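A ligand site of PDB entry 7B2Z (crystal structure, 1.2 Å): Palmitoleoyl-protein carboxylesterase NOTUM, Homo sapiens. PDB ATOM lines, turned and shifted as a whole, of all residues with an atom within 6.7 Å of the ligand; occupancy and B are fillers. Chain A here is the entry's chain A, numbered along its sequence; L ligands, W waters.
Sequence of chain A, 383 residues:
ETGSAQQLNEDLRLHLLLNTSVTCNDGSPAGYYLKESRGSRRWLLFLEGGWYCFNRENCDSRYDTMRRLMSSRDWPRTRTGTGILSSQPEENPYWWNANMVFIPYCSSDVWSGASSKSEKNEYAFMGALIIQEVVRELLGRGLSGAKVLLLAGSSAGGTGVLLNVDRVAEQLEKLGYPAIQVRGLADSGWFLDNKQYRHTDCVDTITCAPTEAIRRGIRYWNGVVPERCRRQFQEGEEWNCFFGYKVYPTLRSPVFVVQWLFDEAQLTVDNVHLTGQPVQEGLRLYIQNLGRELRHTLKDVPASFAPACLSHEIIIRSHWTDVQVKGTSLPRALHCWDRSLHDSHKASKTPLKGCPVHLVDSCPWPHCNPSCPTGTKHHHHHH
N of Trp 51 is in hydrogen-bond range of O1 of the ligand, 2.9 Å away.
N of Ala 156 sits at hydrogen-bond distance from O1 of the ligand (3.0 Å).
An oxygen (O1) of the ligand sits at hydrogen-bond distance from the backbone NH of Gly 50 (2.9 Å).
The side-chain hydroxyl (OG) of Ser 155 is covalently linked to a carbon (C1) of the ligand (1.4 Å).
The backbone carbonyl oxygen of Trp 51 is in hydrogen-bond range of the side-chain hydroxyl of Tyr 105.
O of Gly 189 is in hydrogen-bond range of OG1 of Thr 159, at 2.9 Å.
The backbone carbonyl oxygen (O) of Ser 154 lies close to the backbone NH (N) of Gly 49, at 3.4 Å.
The backbone NH (N) of Ala 265 is in hydrogen-bond range of the side-chain carboxylate (OD1) of Asp 263.
Water W1 lies within hydrogen-bond range of NE2 of His 312 (2.7 Å), O1 of the ligand (3.1 Å) and OG of Ser 155 (3.3 Å).
Merely in contact with the ligand: Gly 49 (3.96 Å), Tyr 52 (3.8 Å), Thr 159 (3.6 Å), Phe 191 (3.3 Å) and Ala 265 (3.5 Å).
Hydrophobic or aromatic side chains that line the ligand: Trp 51, Tyr 52, Ala 156, Phe 191 and Ala 265.
The nearest printed residue that does not touch the ligand is Ile 214 (4.01 Å).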
ATOM      1  N   GLU A  48      -1.018  21.416  29.210  1.00  0.00           N
ATOM      2  CA  GLU A  48      -0.379  22.715  29.189  1.00  0.00           C
ATOM      3  C   GLU A  48       1.021  22.614  28.570  1.00  0.00           C
ATOM      4  O   GLU A  48       1.693  21.582  28.664  1.00  0.00           O
ATOM      5  CB  GLU A  48      -0.281  23.226  30.625  1.00  0.00           C
ATOM      6  CG  GLU A  48       0.293  24.626  30.741  1.00  0.00           C
ATOM      7  CD  GLU A  48       0.507  25.055  32.158  1.00  0.00           C
ATOM      8  OE1 GLU A  48       0.662  24.217  33.070  1.00  0.00           O
ATOM      9  OE2 GLU A  48       0.525  26.293  32.389  1.00  0.00           O
ATOM     10  N   GLY A  49       1.461  23.701  27.937  1.00  0.00           N
ATOM     11  CA  GLY A  49       2.822  23.823  27.456  1.00  0.00           C
ATOM     12  C   GLY A  49       3.698  24.705  28.326  1.00  0.00           C
ATOM     13  O   GLY A  49       3.377  25.060  29.469  1.00  0.00           O
ATOM     14  N   GLY A  50       4.877  25.027  27.778  1.00  0.00           N
ATOM     15  CA  GLY A  50       5.844  25.891  28.439  1.00  0.00           C
ATOM     16  C   GLY A  50       7.283  25.431  28.320  1.00  0.00           C
ATOM     17  O   GLY A  50       7.999  25.351  29.326  1.00  0.00           O
ATOM     18  N   TRP A  51       7.740  25.151  27.103  1.00  0.00           N
ATOM     19  CA  TRP A  51       9.138  24.801  26.812  1.00  0.00           C
ATOM     20  C   TRP A  51       9.491  23.522  27.586  1.00  0.00           C
ATOM     21  O   TRP A  51       8.688  22.580  27.608  1.00  0.00           O
ATOM     22  CB  TRP A  51      10.080  26.000  26.999  1.00  0.00           C
ATOM     23  CG  TRP A  51       9.792  27.093  26.009  1.00  0.00           C
ATOM     24  CD1 TRP A  51       8.924  28.128  26.173  1.00  0.00           C
ATOM     25  CD2 TRP A  51      10.369  27.243  24.695  1.00  0.00           C
ATOM     26  NE1 TRP A  51       8.918  28.916  25.030  1.00  0.00           N
ATOM     27  CE2 TRP A  51       9.796  28.397  24.122  1.00  0.00           C
ATOM     28  CE3 TRP A  51      11.281  26.504  23.958  1.00  0.00           C
ATOM     29  CZ2 TRP A  51      10.142  28.846  22.837  1.00  0.00           C
ATOM     30  CZ3 TRP A  51      11.636  26.956  22.677  1.00  0.00           C
ATOM     31  CH2 TRP A  51      11.060  28.112  22.136  1.00  0.00           C
ATOM     32  N   TYR A  52      10.666  23.458  28.210  1.00  0.00           N
ATOM     33  CA  TYR A  52      11.250  22.242  28.771  1.00  0.00           C
ATOM     34  C   TYR A  52      12.588  22.682  29.371  1.00  0.00           C
ATOM     35  O   TYR A  52      13.027  23.813  29.163  1.00  0.00           O
ATOM     36  CB  TYR A  52      11.475  21.169  27.702  1.00  0.00           C
ATOM     37  CG  TYR A  52      12.013  21.713  26.385  1.00  0.00           C
ATOM     38  CD1 TYR A  52      13.372  21.966  26.231  1.00  0.00           C
ATOM     39  CD2 TYR A  52      11.168  21.970  25.292  1.00  0.00           C
ATOM     40  CE1 TYR A  52      13.874  22.474  25.047  1.00  0.00           C
ATOM     41  CE2 TYR A  52      11.670  22.479  24.108  1.00  0.00           C
ATOM     42  CZ  TYR A  52      13.030  22.721  23.994  1.00  0.00           C
ATOM     43  OH  TYR A  52      13.534  23.217  22.817  1.00  0.00           O
ATOM     44  N   TYR A 105       1.438  21.433  33.310  1.00  0.00           N
ATOM     45  CA  TYR A 105       2.746  20.963  32.884  1.00  0.00           C
ATOM     46  C   TYR A 105       3.745  21.277  33.988  1.00  0.00           C
ATOM     47  O   TYR A 105       4.118  22.433  34.184  1.00  0.00           O
ATOM     48  CB  TYR A 105       3.107  21.701  31.611  1.00  0.00           C
ATOM     49  CG  TYR A 105       4.398  21.328  30.936  1.00  0.00           C
ATOM     50  CD1 TYR A 105       4.830  20.006  30.818  1.00  0.00           C
ATOM     51  CD2 TYR A 105       5.158  22.323  30.310  1.00  0.00           C
ATOM     52  CE1 TYR A 105       5.988  19.703  30.133  1.00  0.00           C
ATOM     53  CE2 TYR A 105       6.296  22.029  29.635  1.00  0.00           C
ATOM     54  CZ  TYR A 105       6.697  20.708  29.534  1.00  0.00           C
ATOM     55  OH  TYR A 105       7.878  20.429  28.853  1.00  0.00           O
ATOM     56  N   VAL A 110       8.414  17.784  27.879  1.00  0.00           N
ATOM     57  CA  VAL A 110       7.534  17.676  26.708  1.00  0.00           C
ATOM     58  C   VAL A 110       6.596  16.479  26.895  1.00  0.00           C
ATOM     59  O   VAL A 110       6.186  15.807  25.933  1.00  0.00           O
ATOM     60  CB  VAL A 110       8.348  17.593  25.392  1.00  0.00           C
ATOM     61  CG1 VAL A 110       7.448  17.840  24.185  1.00  0.00           C
ATOM     62  CG2 VAL A 110       9.527  18.549  25.409  1.00  0.00           C
ATOM     63  N   SER A 154      -1.176  22.455  23.950  1.00  0.00           N
ATOM     64  CA  SER A 154      -0.581  23.591  23.249  1.00  0.00           C
ATOM     65  C   SER A 154       0.928  23.657  23.468  1.00  0.00           C
ATOM     66  O   SER A 154       1.422  23.453  24.587  1.00  0.00           O
ATOM     67  CB  SER A 154      -1.220  24.919  23.678  1.00  0.00           C
ATOM     68  OG  SER A 154      -2.604  24.976  23.326  1.00  0.00           O
ATOM     69  N   SER A 155       1.670  23.995  22.407  1.00  0.00           N
ATOM     70  CA  SER A 155       3.139  24.149  22.445  1.00  0.00           C
ATOM     71  C   SER A 155       3.763  22.819  22.859  1.00  0.00           C
ATOM     72  O   SER A 155       3.511  21.794  22.203  1.00  0.00           O
ATOM     73  CB  SER A 155       3.551  25.386  23.219  1.00  0.00           C
ATOM     74  OG  SER A 155       4.923  25.685  22.889  1.00  0.00           O
ATOM     75  N   ALA A 156       4.567  22.771  23.929  1.00  0.00           N
ATOM     76  CA  ALA A 156       5.097  21.483  24.385  1.00  0.00           C
ATOM     77  C   ALA A 156       3.969  20.501  24.686  1.00  0.00           C
ATOM     78  O   ALA A 156       4.163  19.292  24.565  1.00  0.00           O
ATOM     79  CB  ALA A 156       6.026  21.657  25.593  1.00  0.00           C
ATOM     80  N   GLY A 157       2.806  21.004  25.121  1.00  0.00           N
ATOM     81  CA  GLY A 157       1.662  20.128  25.309  1.00  0.00           C
ATOM     82  C   GLY A 157       1.104  19.591  23.997  1.00  0.00           C
ATOM     83  O   GLY A 157       0.585  18.483  23.967  1.00  0.00           O
ATOM     84  N   THR A 159       3.054  18.903  21.309  1.00  0.00           N
ATOM     85  CA  THR A 159       3.959  17.801  21.038  1.00  0.00           C
ATOM     86  C   THR A 159       3.672  16.631  21.976  1.00  0.00           C
ATOM     87  O   THR A 159       3.692  15.466  21.563  1.00  0.00           O
ATOM     88  CB  THR A 159       5.412  18.257  21.151  1.00  0.00           C
ATOM     89  OG1 THR A 159       5.588  19.500  20.439  1.00  0.00           O
ATOM     90  CG2 THR A 159       6.362  17.185  20.616  1.00  0.00           C
ATOM     91  N   SER A 188       0.114  23.970  18.019  1.00  0.00           N
ATOM     92  CA  SER A 188       1.395  24.673  18.131  1.00  0.00           C
ATOM     93  C   SER A 188       2.490  23.765  18.638  1.00  0.00           C
ATOM     94  O   SER A 188       3.429  24.233  19.297  1.00  0.00           O
ATOM     95  CB  SER A 188       1.260  25.927  18.996  1.00  0.00           C
ATOM     96  OG  SER A 188       0.241  26.782  18.450  1.00  0.00           O
ATOM     97  N   GLY A 189       2.406  22.484  18.298  1.00  0.00           N
ATOM     98  CA  GLY A 189       3.386  21.498  18.683  1.00  0.00           C
ATOM     99  C   GLY A 189       4.018  20.793  17.517  1.00  0.00           C
ATOM    100  O   GLY A 189       4.630  19.738  17.699  1.00  0.00           O
ATOM    101  N   PHE A 191       6.717  21.084  14.898  1.00  0.00           N
ATOM    102  CA  PHE A 191       7.932  21.849  14.659  1.00  0.00           C
ATOM    103  C   PHE A 191       8.797  21.214  13.591  1.00  0.00           C
ATOM    104  O   PHE A 191       8.675  20.030  13.294  1.00  0.00           O
ATOM    105  CB  PHE A 191       8.745  21.965  15.962  1.00  0.00           C
ATOM    106  CG  PHE A 191       8.013  22.686  17.037  1.00  0.00           C
ATOM    107  CD1 PHE A 191       7.778  24.034  16.920  1.00  0.00           C
ATOM    108  CD2 PHE A 191       7.489  22.008  18.148  1.00  0.00           C
ATOM    109  CE1 PHE A 191       7.047  24.714  17.891  1.00  0.00           C
ATOM    110  CE2 PHE A 191       6.776  22.696  19.126  1.00  0.00           C
ATOM    111  CZ  PHE A 191       6.561  24.035  18.998  1.00  0.00           C
ATOM    112  N   PRO A 210      16.945  22.738  18.758  1.00  0.00           N
ATOM    113  CA  PRO A 210      15.975  21.822  19.350  1.00  0.00           C
ATOM    114  C   PRO A 210      16.430  20.374  19.263  1.00  0.00           C
ATOM    115  O   PRO A 210      16.302  19.641  20.235  1.00  0.00           O
ATOM    116  CB  PRO A 210      14.739  22.030  18.474  1.00  0.00           C
ATOM    117  CG  PRO A 210      14.806  23.496  18.138  1.00  0.00           C
ATOM    118  CD  PRO A 210      16.264  23.943  18.248  1.00  0.00           C
ATOM    119  N   THR A 211      16.981  19.987  18.110  1.00  0.00           N
ATOM    120  CA  THR A 211      17.476  18.620  17.943  1.00  0.00           C
ATOM    121  C   THR A 211      18.427  18.238  19.063  1.00  0.00           C
ATOM    122  O   THR A 211      18.222  17.214  19.737  1.00  0.00           O
ATOM    123  CB  THR A 211      18.139  18.454  16.574  1.00  0.00           C
ATOM    124  OG1 THR A 211      19.173  19.433  16.428  1.00  0.00           O
ATOM    125  CG2 THR A 211      17.115  18.623  15.474  1.00  0.00           C
ATOM    126  N   ILE A 214      16.719  18.237  22.566  1.00  0.00           N
ATOM    127  CA  ILE A 214      15.858  17.060  22.712  1.00  0.00           C
ATOM    128  C   ILE A 214      16.686  15.792  22.951  1.00  0.00           C
ATOM    129  O   ILE A 214      16.360  14.984  23.830  1.00  0.00           O
ATOM    130  CB  ILE A 214      14.897  16.925  21.512  1.00  0.00           C
ATOM    131  CG1 ILE A 214      14.004  18.169  21.315  1.00  0.00           C
ATOM    132  CG2 ILE A 214      14.023  15.713  21.674  1.00  0.00           C
ATOM    133  CD1 ILE A 214      13.083  18.498  22.467  1.00  0.00           C
ATOM    134  N   PHE A 242       9.941  13.563  18.284  1.00  0.00           N
ATOM    135  CA  PHE A 242       9.416  14.809  18.813  1.00  0.00           C
ATOM    136  C   PHE A 242       9.019  15.770  17.691  1.00  0.00           C
ATOM    137  O   PHE A 242       8.486  16.852  17.987  1.00  0.00           O
ATOM    138  CB  PHE A 242      10.452  15.483  19.730  1.00  0.00           C
ATOM    139  CG  PHE A 242      10.544  14.868  21.104  1.00  0.00           C
ATOM    140  CD1 PHE A 242      10.955  13.545  21.278  1.00  0.00           C
ATOM    141  CD2 PHE A 242      10.303  15.641  22.236  1.00  0.00           C
ATOM    142  CE1 PHE A 242      11.085  13.003  22.558  1.00  0.00           C
ATOM    143  CE2 PHE A 242      10.425  15.095  23.512  1.00  0.00           C
ATOM    144  CZ  PHE A 242      10.824  13.796  23.661  1.00  0.00           C
ATOM    145  N   PHE A 243       9.261  15.401  16.438  1.00  0.00           N
ATOM    146  CA  PHE A 243       8.965  16.260  15.297  1.00  0.00           C
ATOM    147  C   PHE A 243       7.734  15.734  14.586  1.00  0.00           C
ATOM    148  O   PHE A 243       7.746  14.611  14.056  1.00  0.00           O
ATOM    149  CB  PHE A 243      10.198  16.425  14.411  1.00  0.00           C
ATOM    150  CG  PHE A 243      11.241  17.230  15.096  1.00  0.00           C
ATOM    151  CD1 PHE A 243      11.204  18.602  15.042  1.00  0.00           C
ATOM    152  CD2 PHE A 243      12.154  16.610  15.935  1.00  0.00           C
ATOM    153  CE1 PHE A 243      12.119  19.363  15.749  1.00  0.00           C
ATOM    154  CE2 PHE A 243      13.051  17.343  16.661  1.00  0.00           C
ATOM    155  CZ  PHE A 243      13.035  18.726  16.570  1.00  0.00           C
ATOM    156  N   ASP A 263       5.108  30.038  13.308  1.00  0.00           N
ATOM    157  CA  ASP A 263       4.991  29.956  14.768  1.00  0.00           C
ATOM    158  C   ASP A 263       6.152  30.687  15.448  1.00  0.00           C
ATOM    159  O   ASP A 263       7.322  30.494  15.107  1.00  0.00           O
ATOM    160  CB  ASP A 263       4.952  28.476  15.170  1.00  0.00           C
ATOM    161  CG  ASP A 263       4.756  28.290  16.625  1.00  0.00           C
ATOM    162  OD1 ASP A 263       5.788  28.177  17.343  1.00  0.00           O
ATOM    163  OD2 ASP A 263       3.605  28.274  17.073  1.00  0.00           O
ATOM    164  N   ALA A 265       7.524  30.311  18.339  1.00  0.00           N
ATOM    165  CA  ALA A 265       8.514  29.457  18.989  1.00  0.00           C
ATOM    166  C   ALA A 265       9.430  28.805  17.958  1.00  0.00           C
ATOM    167  O   ALA A 265      10.652  28.664  18.198  1.00  0.00           O
ATOM    168  CB  ALA A 265       7.851  28.428  19.884  1.00  0.00           C
ATOM    169  N   GLN A 266       8.882  28.417  16.807  1.00  0.00           N
ATOM    170  CA  GLN A 266       9.713  27.940  15.699  1.00  0.00           C
ATOM    171  C   GLN A 266      10.726  29.005  15.297  1.00  0.00           C
ATOM    172  O   GLN A 266      11.919  28.715  15.130  1.00  0.00           O
ATOM    173  CB  GLN A 266       8.833  27.562  14.516  1.00  0.00           C
ATOM    174  CG  GLN A 266       9.595  27.100  13.300  1.00  0.00           C
ATOM    175  CD  GLN A 266      10.101  25.675  13.442  1.00  0.00           C
ATOM    176  OE1 GLN A 266       9.327  24.772  13.761  1.00  0.00           O
ATOM    177  NE2 GLN A 266      11.391  25.477  13.189  1.00  0.00           N
ATOM    178  N   VAL A 269      13.547  29.409  17.991  1.00  0.00           N
ATOM    179  CA  VAL A 269      14.593  28.382  17.901  1.00  0.00           C
ATOM    180  C   VAL A 269      15.417  28.542  16.632  1.00  0.00           C
ATOM    181  O   VAL A 269      16.599  28.160  16.601  1.00  0.00           O
ATOM    182  CB  VAL A 269      14.046  26.957  18.133  1.00  0.00           C
ATOM    183  CG1 VAL A 269      13.401  26.840  19.490  1.00  0.00           C
ATOM    184  CG2 VAL A 269      13.049  26.541  17.054  1.00  0.00           C
ATOM    185  N   HIS A 312       1.345  32.220  18.261  1.00  0.00           N
ATOM    186  CA  HIS A 312       1.782  31.092  19.091  1.00  0.00           C
ATOM    187  C   HIS A 312       0.631  30.609  19.964  1.00  0.00           C
ATOM    188  O   HIS A 312       0.137  31.367  20.807  1.00  0.00           O
ATOM    189  CB  HIS A 312       2.960  31.515  19.969  1.00  0.00           C
ATOM    190  CG  HIS A 312       3.494  30.418  20.843  1.00  0.00           C
ATOM    191  ND1 HIS A 312       3.961  29.228  20.336  1.00  0.00           N
ATOM    192  CD2 HIS A 312       3.610  30.337  22.186  1.00  0.00           C
ATOM    193  CE1 HIS A 312       4.357  28.463  21.350  1.00  0.00           C
ATOM    194  NE2 HIS A 312       4.148  29.104  22.468  1.00  0.00           N
ATOM    195  N   GLU A 313       0.278  29.324  19.809  1.00  0.00           N
ATOM    196  CA  GLU A 313      -0.856  28.670  20.484  1.00  0.00           C
ATOM    197  C   GLU A 313      -2.170  29.317  20.035  1.00  0.00           C
ATOM    198  O   GLU A 313      -2.148  30.424  19.489  1.00  0.00           O
ATOM    199  CB  GLU A 313      -0.721  28.664  22.015  1.00  0.00           C
ATOM    200  CG  GLU A 313       0.572  28.031  22.499  1.00  0.00           C
ATOM    201  CD  GLU A 313       0.689  28.078  24.015  1.00  0.00           C
ATOM    202  OE1 GLU A 313       1.204  27.111  24.609  1.00  0.00           O
ATOM    203  OE2 GLU A 313       0.291  29.110  24.593  1.00  0.00           O
HETATM  204  C1  LIG L   1       5.877  25.686  23.879  1.00  0.00           C
HETATM  205  C2  LIG L   1       7.126  26.443  23.445  1.00  0.00           C
HETATM  206  C3  LIG L   1       7.899  25.829  22.290  1.00  0.00           C
HETATM  207  C4  LIG L   1       8.110  24.318  22.303  1.00  0.00           C
HETATM  208  C5  LIG L   1       9.801  24.565  20.391  1.00  0.00           C
HETATM  209  C6  LIG L   1      10.709  23.619  19.668  1.00  0.00           C
HETATM  210  C7  LIG L   1      10.259  22.230  20.088  1.00  0.00           C
HETATM  211  C8  LIG L   1      10.653  20.966  19.612  1.00  0.00           C
HETATM  212  C9  LIG L   1      10.076  19.832  20.175  1.00  0.00           C
HETATM  213  C10 LIG L   1       9.126  19.957  21.194  1.00  0.00           C
HETATM  214  C11 LIG L   1       8.741  21.205  21.665  1.00  0.00           C
HETATM  215  C12 LIG L   1       9.359  22.355  21.128  1.00  0.00           C
HETATM  216  N1  LIG L   1       9.066  23.783  21.361  1.00  0.00           N
HETATM  217  O1  LIG L   1       5.753  25.285  24.987  1.00  0.00           O
HETATM  218  O2  LIG L   1       7.528  23.562  23.029  1.00  0.00           O
HETATM  219  O   HOH W   1       4.973  28.246  24.906  1.00  0.00           O
